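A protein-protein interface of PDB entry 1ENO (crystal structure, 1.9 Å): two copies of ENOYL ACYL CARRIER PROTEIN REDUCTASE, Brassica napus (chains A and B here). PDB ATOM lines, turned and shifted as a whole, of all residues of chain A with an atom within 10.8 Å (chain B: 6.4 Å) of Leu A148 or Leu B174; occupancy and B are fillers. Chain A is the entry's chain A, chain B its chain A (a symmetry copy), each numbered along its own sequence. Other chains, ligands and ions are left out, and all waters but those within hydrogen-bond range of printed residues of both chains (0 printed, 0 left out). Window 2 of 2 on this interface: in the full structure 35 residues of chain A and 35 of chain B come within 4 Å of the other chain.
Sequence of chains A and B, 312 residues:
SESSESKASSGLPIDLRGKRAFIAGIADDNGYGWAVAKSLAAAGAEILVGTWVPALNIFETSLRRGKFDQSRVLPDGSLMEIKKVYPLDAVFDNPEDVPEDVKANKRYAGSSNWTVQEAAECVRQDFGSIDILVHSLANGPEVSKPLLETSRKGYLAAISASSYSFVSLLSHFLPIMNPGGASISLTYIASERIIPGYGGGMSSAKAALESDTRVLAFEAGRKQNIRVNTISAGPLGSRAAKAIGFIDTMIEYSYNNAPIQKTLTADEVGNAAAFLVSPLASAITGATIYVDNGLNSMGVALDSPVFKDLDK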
ATOM      1  N   GLU A 142     -10.720 -16.001  -4.904  1.00  0.00           N
ATOM      2  CA  GLU A 142     -11.042 -15.515  -6.260  1.00  0.00           C
ATOM      3  C   GLU A 142     -10.101 -14.404  -6.736  1.00  0.00           C
ATOM      4  O   GLU A 142     -10.485 -13.507  -7.506  1.00  0.00           O
ATOM      5  CB  GLU A 142     -12.526 -15.080  -6.412  1.00  0.00           C
ATOM      6  CG  GLU A 142     -13.499 -16.235  -6.093  1.00  0.00           C
ATOM      7  CD  GLU A 142     -14.957 -15.891  -6.090  1.00  0.00           C
ATOM      8  OE1 GLU A 142     -15.238 -14.882  -6.729  1.00  0.00           O
ATOM      9  OE2 GLU A 142     -15.791 -16.534  -5.437  1.00  0.00           O
ATOM     10  N   VAL A 143      -8.878 -14.440  -6.255  1.00  0.00           N
ATOM     11  CA  VAL A 143      -7.958 -13.371  -6.543  1.00  0.00           C
ATOM     12  C   VAL A 143      -7.721 -13.132  -8.011  1.00  0.00           C
ATOM     13  O   VAL A 143      -7.393 -12.044  -8.430  1.00  0.00           O
ATOM     14  CB  VAL A 143      -6.687 -13.511  -5.783  1.00  0.00           C
ATOM     15  CG1 VAL A 143      -5.899 -14.650  -6.413  1.00  0.00           C
ATOM     16  CG2 VAL A 143      -5.927 -12.196  -5.896  1.00  0.00           C
ATOM     17  N   SER A 144      -7.925 -14.128  -8.833  1.00  0.00           N
ATOM     18  CA  SER A 144      -7.726 -13.893 -10.263  1.00  0.00           C
ATOM     19  C   SER A 144      -8.913 -13.252 -11.014  1.00  0.00           C
ATOM     20  O   SER A 144      -8.796 -12.909 -12.168  1.00  0.00           O
ATOM     21  CB  SER A 144      -7.260 -15.137 -10.959  1.00  0.00           C
ATOM     22  OG  SER A 144      -8.268 -16.114 -10.856  1.00  0.00           O
ATOM     23  N   LYS A 145     -10.054 -13.099 -10.374  1.00  0.00           N
ATOM     24  CA  LYS A 145     -11.261 -12.509 -10.968  1.00  0.00           C
ATOM     25  C   LYS A 145     -11.376 -10.966 -10.757  1.00  0.00           C
ATOM     26  O   LYS A 145     -11.059 -10.429  -9.713  1.00  0.00           O
ATOM     27  CB  LYS A 145     -12.524 -13.156 -10.396  1.00  0.00           C
ATOM     28  CG  LYS A 145     -12.521 -14.683 -10.429  1.00  0.00           C
ATOM     29  CD  LYS A 145     -13.825 -15.300 -10.917  1.00  0.00           C
ATOM     30  CE  LYS A 145     -13.631 -16.551 -11.783  1.00  0.00           C
ATOM     31  NZ  LYS A 145     -12.737 -17.568 -11.187  1.00  0.00           N
ATOM     32  N   PRO A 146     -11.943 -10.265 -11.712  1.00  0.00           N
ATOM     33  CA  PRO A 146     -12.188  -8.851 -11.522  1.00  0.00           C
ATOM     34  C   PRO A 146     -13.261  -8.704 -10.481  1.00  0.00           C
ATOM     35  O   PRO A 146     -14.012  -9.653 -10.268  1.00  0.00           O
ATOM     36  CB  PRO A 146     -12.812  -8.308 -12.819  1.00  0.00           C
ATOM     37  CG  PRO A 146     -12.869  -9.468 -13.785  1.00  0.00           C
ATOM     38  CD  PRO A 146     -12.211 -10.675 -13.105  1.00  0.00           C
ATOM     39  N   LEU A 147     -13.397  -7.500  -9.902  1.00  0.00           N
ATOM     40  CA  LEU A 147     -14.426  -7.318  -8.918  1.00  0.00           C
ATOM     41  C   LEU A 147     -15.784  -7.648  -9.503  1.00  0.00           C
ATOM     42  O   LEU A 147     -16.625  -8.209  -8.838  1.00  0.00           O
ATOM     43  CB  LEU A 147     -14.480  -5.867  -8.362  1.00  0.00           C
ATOM     44  CG  LEU A 147     -13.598  -5.608  -7.190  1.00  0.00           C
ATOM     45  CD1 LEU A 147     -13.882  -4.194  -6.682  1.00  0.00           C
ATOM     46  CD2 LEU A 147     -13.823  -6.616  -6.086  1.00  0.00           C
ATOM     47  N   LEU A 148     -16.009  -7.183 -10.740  1.00  0.00           N
ATOM     48  CA  LEU A 148     -17.289  -7.385 -11.386  1.00  0.00           C
ATOM     49  C   LEU A 148     -17.655  -8.875 -11.440  1.00  0.00           C
ATOM     50  O   LEU A 148     -18.806  -9.226 -11.611  1.00  0.00           O
ATOM     51  CB  LEU A 148     -17.328  -6.744 -12.817  1.00  0.00           C
ATOM     52  CG  LEU A 148     -17.515  -5.211 -12.857  1.00  0.00           C
ATOM     53  CD1 LEU A 148     -17.633  -4.756 -14.315  1.00  0.00           C
ATOM     54  CD2 LEU A 148     -18.784  -4.833 -12.091  1.00  0.00           C
ATOM     55  N   GLU A 149     -16.666  -9.739 -11.309  1.00  0.00           N
ATOM     56  CA  GLU A 149     -16.928 -11.183 -11.406  1.00  0.00           C
ATOM     57  C   GLU A 149     -16.737 -11.903 -10.109  1.00  0.00           C
ATOM     58  O   GLU A 149     -16.843 -13.095 -10.105  1.00  0.00           O
ATOM     59  CB  GLU A 149     -16.033 -11.860 -12.461  1.00  0.00           C
ATOM     60  CG  GLU A 149     -16.493 -11.463 -13.891  1.00  0.00           C
ATOM     61  CD  GLU A 149     -15.525 -11.823 -14.997  1.00  0.00           C
ATOM     62  OE1 GLU A 149     -14.759 -12.823 -14.960  1.00  0.00           O
ATOM     63  OE2 GLU A 149     -15.535 -10.978 -15.923  1.00  0.00           O
ATOM     64  N   THR A 150     -16.407 -11.184  -9.028  1.00  0.00           N
ATOM     65  CA  THR A 150     -16.184 -11.799  -7.712  1.00  0.00           C
ATOM     66  C   THR A 150     -17.468 -12.117  -6.933  1.00  0.00           C
ATOM     67  O   THR A 150     -18.353 -11.294  -6.803  1.00  0.00           O
ATOM     68  CB  THR A 150     -15.233 -10.924  -6.874  1.00  0.00           C
ATOM     69  OG1 THR A 150     -14.013 -10.828  -7.612  1.00  0.00           O
ATOM     70  CG2 THR A 150     -14.986 -11.555  -5.482  1.00  0.00           C
ATOM     71  N   SER A 151     -17.570 -13.320  -6.372  1.00  0.00           N
ATOM     72  CA  SER A 151     -18.787 -13.627  -5.617  1.00  0.00           C
ATOM     73  C   SER A 151     -18.718 -13.079  -4.210  1.00  0.00           C
ATOM     74  O   SER A 151     -17.651 -12.752  -3.708  1.00  0.00           O
ATOM     75  CB  SER A 151     -19.100 -15.114  -5.576  1.00  0.00           C
ATOM     76  OG  SER A 151     -18.179 -15.733  -4.669  1.00  0.00           O
ATOM     77  N   ARG A 152     -19.894 -12.962  -3.589  1.00  0.00           N
ATOM     78  CA  ARG A 152     -19.966 -12.444  -2.245  1.00  0.00           C
ATOM     79  C   ARG A 152     -19.093 -13.302  -1.343  1.00  0.00           C
ATOM     80  O   ARG A 152     -18.362 -12.821  -0.501  1.00  0.00           O
ATOM     81  CB  ARG A 152     -21.412 -12.470  -1.740  1.00  0.00           C
ATOM     82  CG  ARG A 152     -21.594 -11.796  -0.366  1.00  0.00           C
ATOM     83  CD  ARG A 152     -23.078 -11.616   0.069  1.00  0.00           C
ATOM     84  NE  ARG A 152     -23.830 -10.799  -0.871  1.00  0.00           N
ATOM     85  CZ  ARG A 152     -24.196  -9.543  -0.688  1.00  0.00           C
ATOM     86  NH1 ARG A 152     -23.926  -8.886   0.441  1.00  0.00           N
ATOM     87  NH2 ARG A 152     -24.851  -8.925  -1.677  1.00  0.00           N
ATOM     88  N   TYR A 155     -15.463 -12.690  -2.017  1.00  0.00           N
ATOM     89  CA  TYR A 155     -15.105 -11.381  -1.477  1.00  0.00           C
ATOM     90  C   TYR A 155     -14.939 -11.404   0.079  1.00  0.00           C
ATOM     91  O   TYR A 155     -13.936 -10.995   0.652  1.00  0.00           O
ATOM     92  CB  TYR A 155     -16.148 -10.368  -1.976  1.00  0.00           C
ATOM     93  CG  TYR A 155     -15.895  -8.896  -1.632  1.00  0.00           C
ATOM     94  CD1 TYR A 155     -16.199  -8.386  -0.362  1.00  0.00           C
ATOM     95  CD2 TYR A 155     -15.413  -8.007  -2.604  1.00  0.00           C
ATOM     96  CE1 TYR A 155     -16.147  -7.001  -0.092  1.00  0.00           C
ATOM     97  CE2 TYR A 155     -15.351  -6.630  -2.358  1.00  0.00           C
ATOM     98  CZ  TYR A 155     -15.730  -6.124  -1.106  1.00  0.00           C
ATOM     99  OH  TYR A 155     -15.666  -4.771  -0.847  1.00  0.00           O
ATOM    100  N   GLY A 197      -5.725  -6.878 -12.114  1.00  0.00           N
ATOM    101  CA  GLY A 197      -5.162  -8.175 -11.864  1.00  0.00           C
ATOM    102  C   GLY A 197      -5.062  -8.525 -10.398  1.00  0.00           C
ATOM    103  O   GLY A 197      -4.787  -9.634 -10.061  1.00  0.00           O
ATOM    104  N   TYR A 198      -5.265  -7.575  -9.516  1.00  0.00           N
ATOM    105  CA  TYR A 198      -5.233  -7.888  -8.084  1.00  0.00           C
ATOM    106  C   TYR A 198      -6.699  -7.992  -7.671  1.00  0.00           C
ATOM    107  O   TYR A 198      -7.319  -7.026  -7.221  1.00  0.00           O
ATOM    108  CB  TYR A 198      -4.521  -6.753  -7.354  1.00  0.00           C
ATOM    109  CG  TYR A 198      -4.069  -7.113  -5.951  1.00  0.00           C
ATOM    110  CD1 TYR A 198      -2.979  -7.955  -5.718  1.00  0.00           C
ATOM    111  CD2 TYR A 198      -4.747  -6.585  -4.849  1.00  0.00           C
ATOM    112  CE1 TYR A 198      -2.591  -8.263  -4.405  1.00  0.00           C
ATOM    113  CE2 TYR A 198      -4.352  -6.841  -3.534  1.00  0.00           C
ATOM    114  CZ  TYR A 198      -3.265  -7.686  -3.327  1.00  0.00           C
ATOM    115  OH  TYR A 198      -2.852  -7.943  -2.062  1.00  0.00           O
ATOM    116  N   GLY A 199      -7.312  -9.145  -7.979  1.00  0.00           N
ATOM    117  CA  GLY A 199      -8.746  -9.281  -7.890  1.00  0.00           C
ATOM    118  C   GLY A 199      -9.276  -9.931  -6.675  1.00  0.00           C
ATOM    119  O   GLY A 199      -8.618 -10.023  -5.671  1.00  0.00           O
ATOM    120  N   GLY A 200     -10.523 -10.348  -6.809  1.00  0.00           N
ATOM    121  CA  GLY A 200     -11.207 -11.110  -5.821  1.00  0.00           C
ATOM    122  C   GLY A 200     -11.461 -10.407  -4.489  1.00  0.00           C
ATOM    123  O   GLY A 200     -11.694 -11.071  -3.496  1.00  0.00           O
ATOM    124  N   GLY A 201     -11.442  -9.091  -4.435  1.00  0.00           N
ATOM    125  CA  GLY A 201     -11.671  -8.421  -3.149  1.00  0.00           C
ATOM    126  C   GLY A 201     -10.395  -8.330  -2.333  1.00  0.00           C
ATOM    127  O   GLY A 201     -10.441  -7.978  -1.154  1.00  0.00           O
ATOM    128  N   MET A 202      -9.239  -8.695  -2.937  1.00  0.00           N
ATOM    129  CA  MET A 202      -7.982  -8.583  -2.217  1.00  0.00           C
ATOM    130  C   MET A 202      -7.610  -7.091  -2.100  1.00  0.00           C
ATOM    131  O   MET A 202      -7.028  -6.624  -1.115  1.00  0.00           O
ATOM    132  CB  MET A 202      -6.836  -9.393  -2.897  1.00  0.00           C
ATOM    133  CG  MET A 202      -6.857 -10.864  -2.572  1.00  0.00           C
ATOM    134  SD  MET A 202      -6.595 -11.171  -0.795  1.00  0.00           S
ATOM    135  CE  MET A 202      -5.363  -9.918  -0.487  1.00  0.00           C
ATOM    136  N   SER A 203      -7.978  -6.302  -3.133  1.00  0.00           N
ATOM    137  CA  SER A 203      -7.692  -4.881  -3.009  1.00  0.00           C
ATOM    138  C   SER A 203      -8.550  -4.304  -1.835  1.00  0.00           C
ATOM    139  O   SER A 203      -8.068  -3.532  -0.990  1.00  0.00           O
ATOM    140  CB  SER A 203      -8.008  -4.187  -4.303  1.00  0.00           C
ATOM    141  OG  SER A 203      -9.362  -4.458  -4.626  1.00  0.00           O
ATOM    142  N   SER A 204      -9.837  -4.752  -1.792  1.00  0.00           N
ATOM    143  CA  SER A 204     -10.796  -4.383  -0.779  1.00  0.00           C
ATOM    144  C   SER A 204     -10.258  -4.706   0.594  1.00  0.00           C
ATOM    145  O   SER A 204     -10.349  -3.895   1.547  1.00  0.00           O
ATOM    146  CB  SER A 204     -12.099  -5.113  -1.030  1.00  0.00           C
ATOM    147  OG  SER A 204     -12.330  -5.166  -2.435  1.00  0.00           O
ATOM    148  N   LEU B 133     -27.349   4.695 -11.065  1.00  0.00           N
ATOM    149  CA  LEU B 133     -27.459   3.806  -9.919  1.00  0.00           C
ATOM    150  C   LEU B 133     -26.979   4.529  -8.680  1.00  0.00           C
ATOM    151  O   LEU B 133     -25.850   5.001  -8.643  1.00  0.00           O
ATOM    152  CB  LEU B 133     -26.555   2.579 -10.134  1.00  0.00           C
ATOM    153  CG  LEU B 133     -26.653   1.560  -8.975  1.00  0.00           C
ATOM    154  CD1 LEU B 133     -28.088   1.049  -8.866  1.00  0.00           C
ATOM    155  CD2 LEU B 133     -25.750   0.343  -9.296  1.00  0.00           C
ATOM    156  N   VAL B 167     -20.935  -3.698  -4.907  1.00  0.00           N
ATOM    157  CA  VAL B 167     -20.387  -4.533  -5.970  1.00  0.00           C
ATOM    158  C   VAL B 167     -21.504  -5.366  -6.642  1.00  0.00           C
ATOM    159  O   VAL B 167     -21.614  -5.462  -7.873  1.00  0.00           O
ATOM    160  CB  VAL B 167     -19.232  -5.439  -5.456  1.00  0.00           C
ATOM    161  CG1 VAL B 167     -18.699  -6.328  -6.591  1.00  0.00           C
ATOM    162  CG2 VAL B 167     -18.081  -4.585  -4.897  1.00  0.00           C
ATOM    163  N   LEU B 169     -24.841  -4.879  -6.602  1.00  0.00           N
ATOM    164  CA  LEU B 169     -25.801  -4.057  -7.332  1.00  0.00           C
ATOM    165  C   LEU B 169     -25.294  -3.662  -8.697  1.00  0.00           C
ATOM    166  O   LEU B 169     -25.962  -3.822  -9.720  1.00  0.00           O
ATOM    167  CB  LEU B 169     -26.199  -2.802  -6.502  1.00  0.00           C
ATOM    168  CG  LEU B 169     -27.216  -3.170  -5.435  1.00  0.00           C
ATOM    169  CD1 LEU B 169     -27.242  -2.121  -4.349  1.00  0.00           C
ATOM    170  CD2 LEU B 169     -28.602  -3.370  -6.048  1.00  0.00           C
ATOM    171  N   LEU B 170     -24.067  -3.112  -8.705  1.00  0.00           N
ATOM    172  CA  LEU B 170     -23.440  -2.648  -9.939  1.00  0.00           C
ATOM    173  C   LEU B 170     -23.331  -3.789 -10.962  1.00  0.00           C
ATOM    174  O   LEU B 170     -23.576  -3.661 -12.175  1.00  0.00           O
ATOM    175  CB  LEU B 170     -22.007  -2.062  -9.639  1.00  0.00           C
ATOM    176  CG  LEU B 170     -21.378  -1.459 -10.896  1.00  0.00           C
ATOM    177  CD1 LEU B 170     -22.316  -0.405 -11.510  1.00  0.00           C
ATOM    178  CD2 LEU B 170     -19.983  -0.880 -10.611  1.00  0.00           C
ATOM    179  N   SER B 171     -22.815  -4.889 -10.479  1.00  0.00           N
ATOM    180  CA  SER B 171     -22.597  -6.029 -11.284  1.00  0.00           C
ATOM    181  C   SER B 171     -23.897  -6.584 -11.916  1.00  0.00           C
ATOM    182  O   SER B 171     -23.943  -6.986 -13.084  1.00  0.00           O
ATOM    183  CB  SER B 171     -21.857  -7.023 -10.427  1.00  0.00           C
ATOM    184  OG  SER B 171     -21.513  -8.094 -11.164  1.00  0.00           O
ATOM    185  N   HIS B 172     -24.950  -6.603 -11.154  1.00  0.00           N
ATOM    186  CA  HIS B 172     -26.203  -7.131 -11.636  1.00  0.00           C
ATOM    187  C   HIS B 172     -26.926  -6.134 -12.499  1.00  0.00           C
ATOM    188  O   HIS B 172     -27.661  -6.500 -13.391  1.00  0.00           O
ATOM    189  CB  HIS B 172     -27.117  -7.590 -10.485  1.00  0.00           C
ATOM    190  CG  HIS B 172     -26.748  -8.948  -9.912  1.00  0.00           C
ATOM    191  ND1 HIS B 172     -25.937  -9.066  -8.779  1.00  0.00           N
ATOM    192  CD2 HIS B 172     -27.113 -10.212 -10.291  1.00  0.00           C
ATOM    193  CE1 HIS B 172     -25.817 -10.370  -8.529  1.00  0.00           C
ATOM    194  NE2 HIS B 172     -26.526 -11.071  -9.403  1.00  0.00           N
ATOM    195  N   PHE B 173     -26.765  -4.856 -12.215  1.00  0.00           N
ATOM    196  CA  PHE B 173     -27.450  -3.861 -13.031  1.00  0.00           C
ATOM    197  C   PHE B 173     -26.684  -3.466 -14.297  1.00  0.00           C
ATOM    198  O   PHE B 173     -27.271  -2.996 -15.272  1.00  0.00           O
ATOM    199  CB  PHE B 173     -27.746  -2.608 -12.201  1.00  0.00           C
ATOM    200  CG  PHE B 173     -29.020  -2.708 -11.439  1.00  0.00           C
ATOM    201  CD1 PHE B 173     -30.228  -2.301 -12.009  1.00  0.00           C
ATOM    202  CD2 PHE B 173     -29.046  -3.246 -10.154  1.00  0.00           C
ATOM    203  CE1 PHE B 173     -31.430  -2.394 -11.301  1.00  0.00           C
ATOM    204  CE2 PHE B 173     -30.244  -3.359  -9.439  1.00  0.00           C
ATOM    205  CZ  PHE B 173     -31.434  -2.911 -10.008  1.00  0.00           C
ATOM    206  N   LEU B 174     -25.368  -3.613 -14.280  1.00  0.00           N
ATOM    207  CA  LEU B 174     -24.543  -3.166 -15.414  1.00  0.00           C
ATOM    208  C   LEU B 174     -25.063  -3.525 -16.822  1.00  0.00           C
ATOM    209  O   LEU B 174     -24.983  -2.753 -17.778  1.00  0.00           O
ATOM    210  CB  LEU B 174     -23.103  -3.655 -15.247  1.00  0.00           C
ATOM    211  CG  LEU B 174     -22.127  -2.880 -16.107  1.00  0.00           C
ATOM    212  CD1 LEU B 174     -22.004  -1.460 -15.595  1.00  0.00           C
ATOM    213  CD2 LEU B 174     -20.757  -3.539 -16.084  1.00  0.00           C
ATOM    214  N   PRO B 175     -25.554  -4.703 -16.969  1.00  0.00           N
ATOM    215  CA  PRO B 175     -26.028  -5.125 -18.264  1.00  0.00           C
ATOM    216  C   PRO B 175     -27.193  -4.334 -18.735  1.00  0.00           C
ATOM    217  O   PRO B 175     -27.481  -4.306 -19.913  1.00  0.00           O
ATOM    218  CB  PRO B 175     -26.479  -6.558 -18.137  1.00  0.00           C
ATOM    219  CG  PRO B 175     -26.148  -6.994 -16.722  1.00  0.00           C
ATOM    220  CD  PRO B 175     -25.549  -5.808 -16.006  1.00  0.00           C
ATOM    221  N   ILE B 176     -27.906  -3.734 -17.819  1.00  0.00           N
ATOM    222  CA  ILE B 176     -29.038  -2.911 -18.248  1.00  0.00           C
ATOM    223  C   ILE B 176     -28.822  -1.404 -18.109  1.00  0.00           C
ATOM    224  O   ILE B 176     -29.761  -0.608 -18.224  1.00  0.00           O
ATOM    225  CB  ILE B 176     -30.363  -3.376 -17.719  1.00  0.00           C
ATOM    226  CG1 ILE B 176     -30.442  -3.171 -16.224  1.00  0.00           C
ATOM    227  CG2 ILE B 176     -30.496  -4.836 -18.023  1.00  0.00           C
ATOM    228  CD1 ILE B 176     -31.864  -3.039 -15.748  1.00  0.00           C
ATOM    229  N   MET B 177     -27.563  -0.997 -17.875  1.00  0.00           N
ATOM    230  CA  MET B 177     -27.258   0.411 -17.778  1.00  0.00           C
ATOM    231  C   MET B 177     -26.824   0.931 -19.112  1.00  0.00           C
ATOM    232  O   MET B 177     -25.940   0.359 -19.744  1.00  0.00           O
ATOM    233  CB  MET B 177     -26.141   0.698 -16.739  1.00  0.00           C
ATOM    234  CG  MET B 177     -26.622   0.572 -15.302  1.00  0.00           C
ATOM    235  SD  MET B 177     -25.275   0.923 -14.118  1.00  0.00           S
ATOM    236  CE  MET B 177     -25.397   2.731 -13.983  1.00  0.00           C
ATOM    237  N   ASN B 178     -27.369   2.064 -19.500  1.00  0.00           N
ATOM    238  CA  ASN B 178     -26.982   2.652 -20.765  1.00  0.00           C
ATOM    239  C   ASN B 178     -25.601   3.265 -20.657  1.00  0.00           C
ATOM    240  O   ASN B 178     -25.321   3.970 -19.688  1.00  0.00           O
ATOM    241  CB  ASN B 178     -27.965   3.749 -21.113  1.00  0.00           C
ATOM    242  CG  ASN B 178     -29.378   3.210 -21.322  1.00  0.00           C
ATOM    243  OD1 ASN B 178     -29.528   2.216 -21.974  1.00  0.00           O
ATOM    244  ND2 ASN B 178     -30.407   3.868 -20.769  1.00  0.00           N
ATOM    245  N   LEU B 216     -13.851  -0.312  -9.597  1.00  0.00           N
ATOM    246  CA  LEU B 216     -15.013  -0.407 -10.470  1.00  0.00           C
ATOM    247  C   LEU B 216     -15.058   0.721 -11.519  1.00  0.00           C
ATOM    248  O   LEU B 216     -15.589   0.520 -12.618  1.00  0.00           O
ATOM    249  CB  LEU B 216     -16.303  -0.513  -9.665  1.00  0.00           C
ATOM    250  CG  LEU B 216     -16.303  -1.777  -8.797  1.00  0.00           C
ATOM    251  CD1 LEU B 216     -17.473  -1.722  -7.795  1.00  0.00           C
ATOM    252  CD2 LEU B 216     -16.434  -2.999  -9.716  1.00  0.00           C
ATOM    253  N   GLU B 219     -13.021  -0.932 -14.109  1.00  0.00           N
ATOM    254  CA  GLU B 219     -13.731  -2.066 -14.706  1.00  0.00           C
ATOM    255  C   GLU B 219     -14.951  -1.705 -15.524  1.00  0.00           C
ATOM    256  O   GLU B 219     -15.129  -2.188 -16.650  1.00  0.00           O
ATOM    257  CB  GLU B 219     -14.019  -3.232 -13.747  1.00  0.00           C
ATOM    258  CG  GLU B 219     -12.806  -3.689 -12.928  1.00  0.00           C
ATOM    259  CD  GLU B 219     -13.078  -4.917 -12.039  1.00  0.00           C
ATOM    260  OE1 GLU B 219     -14.213  -5.478 -12.201  1.00  0.00           O
ATOM    261  OE2 GLU B 219     -12.206  -5.361 -11.298  1.00  0.00           O
ATOM    262  N   ALA B 220     -15.817  -0.903 -14.953  1.00  0.00           N
ATOM    263  CA  ALA B 220     -17.027  -0.484 -15.631  1.00  0.00           C
ATOM    264  C   ALA B 220     -16.798   0.635 -16.616  1.00  0.00           C
ATOM    265  O   ALA B 220     -17.531   0.783 -17.600  1.00  0.00           O
ATOM    266  CB  ALA B 220     -18.075  -0.092 -14.628  1.00  0.00           C
ATOM    267  N   LYS B 223     -15.466  -1.179 -19.553  1.00  0.00           N
ATOM    268  CA  LYS B 223     -16.394  -2.149 -20.056  1.00  0.00           C
ATOM    269  C   LYS B 223     -17.623  -1.562 -20.664  1.00  0.00           C
ATOM    270  O   LYS B 223     -18.098  -2.022 -21.702  1.00  0.00           O
ATOM    271  CB  LYS B 223     -16.741  -3.215 -19.047  1.00  0.00           C
ATOM    272  CG  LYS B 223     -17.937  -4.045 -19.469  1.00  0.00           C
ATOM    273  CD  LYS B 223     -18.296  -5.086 -18.427  1.00  0.00           C
ATOM    274  CE  LYS B 223     -18.081  -6.527 -18.887  1.00  0.00           C
ATOM    275  NZ  LYS B 223     -18.984  -6.943 -19.972  1.00  0.00           N
ATOM    276  N   GLN B 224     -18.154  -0.558 -20.033  1.00  0.00           N
ATOM    277  CA  GLN B 224     -19.394  -0.037 -20.530  1.00  0.00           C
ATOM    278  C   GLN B 224     -19.476   1.499 -20.567  1.00  0.00           C
ATOM    279  O   GLN B 224     -20.563   2.073 -20.795  1.00  0.00           O
ATOM    280  CB  GLN B 224     -20.446  -0.668 -19.620  1.00  0.00           C
ATOM    281  CG  GLN B 224     -21.868  -0.269 -19.977  1.00  0.00           C
ATOM    282  CD  GLN B 224     -22.759  -1.461 -19.984  1.00  0.00           C
ATOM    283  OE1 GLN B 224     -22.285  -2.588 -19.768  1.00  0.00           O
ATOM    284  NE2 GLN B 224     -23.998  -1.248 -20.396  1.00  0.00           N
ATOM    285  N   ILE B 226     -19.218   3.632 -18.086  1.00  0.00           N
ATOM    286  CA  ILE B 226     -19.997   4.058 -16.924  1.00  0.00           C
ATOM    287  C   ILE B 226     -19.057   4.723 -15.911  1.00  0.00           C
ATOM    288  O   ILE B 226     -17.983   4.171 -15.602  1.00  0.00           O
ATOM    289  CB  ILE B 226     -20.631   2.812 -16.269  1.00  0.00           C
ATOM    290  CG1 ILE B 226     -21.585   2.087 -17.258  1.00  0.00           C
ATOM    291  CG2 ILE B 226     -21.316   3.134 -14.877  1.00  0.00           C
ATOM    292  CD1 ILE B 226     -22.805   2.900 -17.642  1.00  0.00           C
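The side-chain carboxylate of Glu B219 sits at hydrogen-bond distance from the backbone NH of Leu A148. The backbone carbonyl oxygen (O) of Leu A148 sits at hydrogen-bond distance from the side-chain hydroxyl (OG) of Ser B171 (3.0 Å). The backbone NH (N) of Leu A147 is in hydrogen-bond range of the side-chain carboxylate (OE2) of Glu B219 (2.8 Å).
Of the printed residues of chain B, Pro A146 touches Glu B219 (3.2 Å). Leu A148 touches just these residues of chain B: Ser B171, Leu B174, Leu B216 and Glu B219. Tyr A155 touches none of the printed residues of chain B. Of the printed residues of chain A, Val B167 touches Leu A147 (3.6 Å). Leu B174 touches one residue of chain A. No residue of chain A comes within 4 Å of Pro B175. No residue of chain A comes within 4 Å of Ile B176. No residue of chain A comes within 4 Å of Met B177. Asn B178 touches none of the printed residues of chain A. Printed residues of chain A within 4 Å of Leu B216: Leu A147 and Leu A148. Glu B219 touches just these residues of chain A: Pro A146 (3.2 Å), Leu A147 (2.8 Å) and Leu A148 (2.9 Å). No residue of chain A comes within 4 Å of Ala B220. No residue of chain A comes within 4 Å of Lys B223. No residue of chain A comes within 4 Å of Gln B224. The nearest residue of chain B that does not touch Leu A148 is Lys B223 (4.2 Å). The nearest residue of chain A that does not touch Leu B174 is Glu A149 (8.8 Å).
No position is printed for both chains. Of the 8 pairs that touch across the chains among the printed residues, none has its exchanged pair printed and touching as well.
Among the printed residues, pairs that only touch across the chains: Pro A146 with Glu B219, Leu A147 with Val B167, Leu A147 with Leu B216, Leu A148 with Leu B174 and Leu A148 with Leu B216.
Hydrophobic or aromatic side chains of chain A within 4 Å of the printed part of chain B: Pro A146, Leu A147 and Leu A148. Among the printed residues, no Asp or Glu carboxylate lies within 4 Å of a Lys or Arg side-chain nitrogen of the other chain.
O of Leu B174 lies within hydrogen-bond range of NE2 of Gln B224 (3.2 Å). The side-chain hydroxyl (OG1) of Thr A150 sits at hydrogen-bond distance from the backbone carbonyl oxygen (O) of Pro A146.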
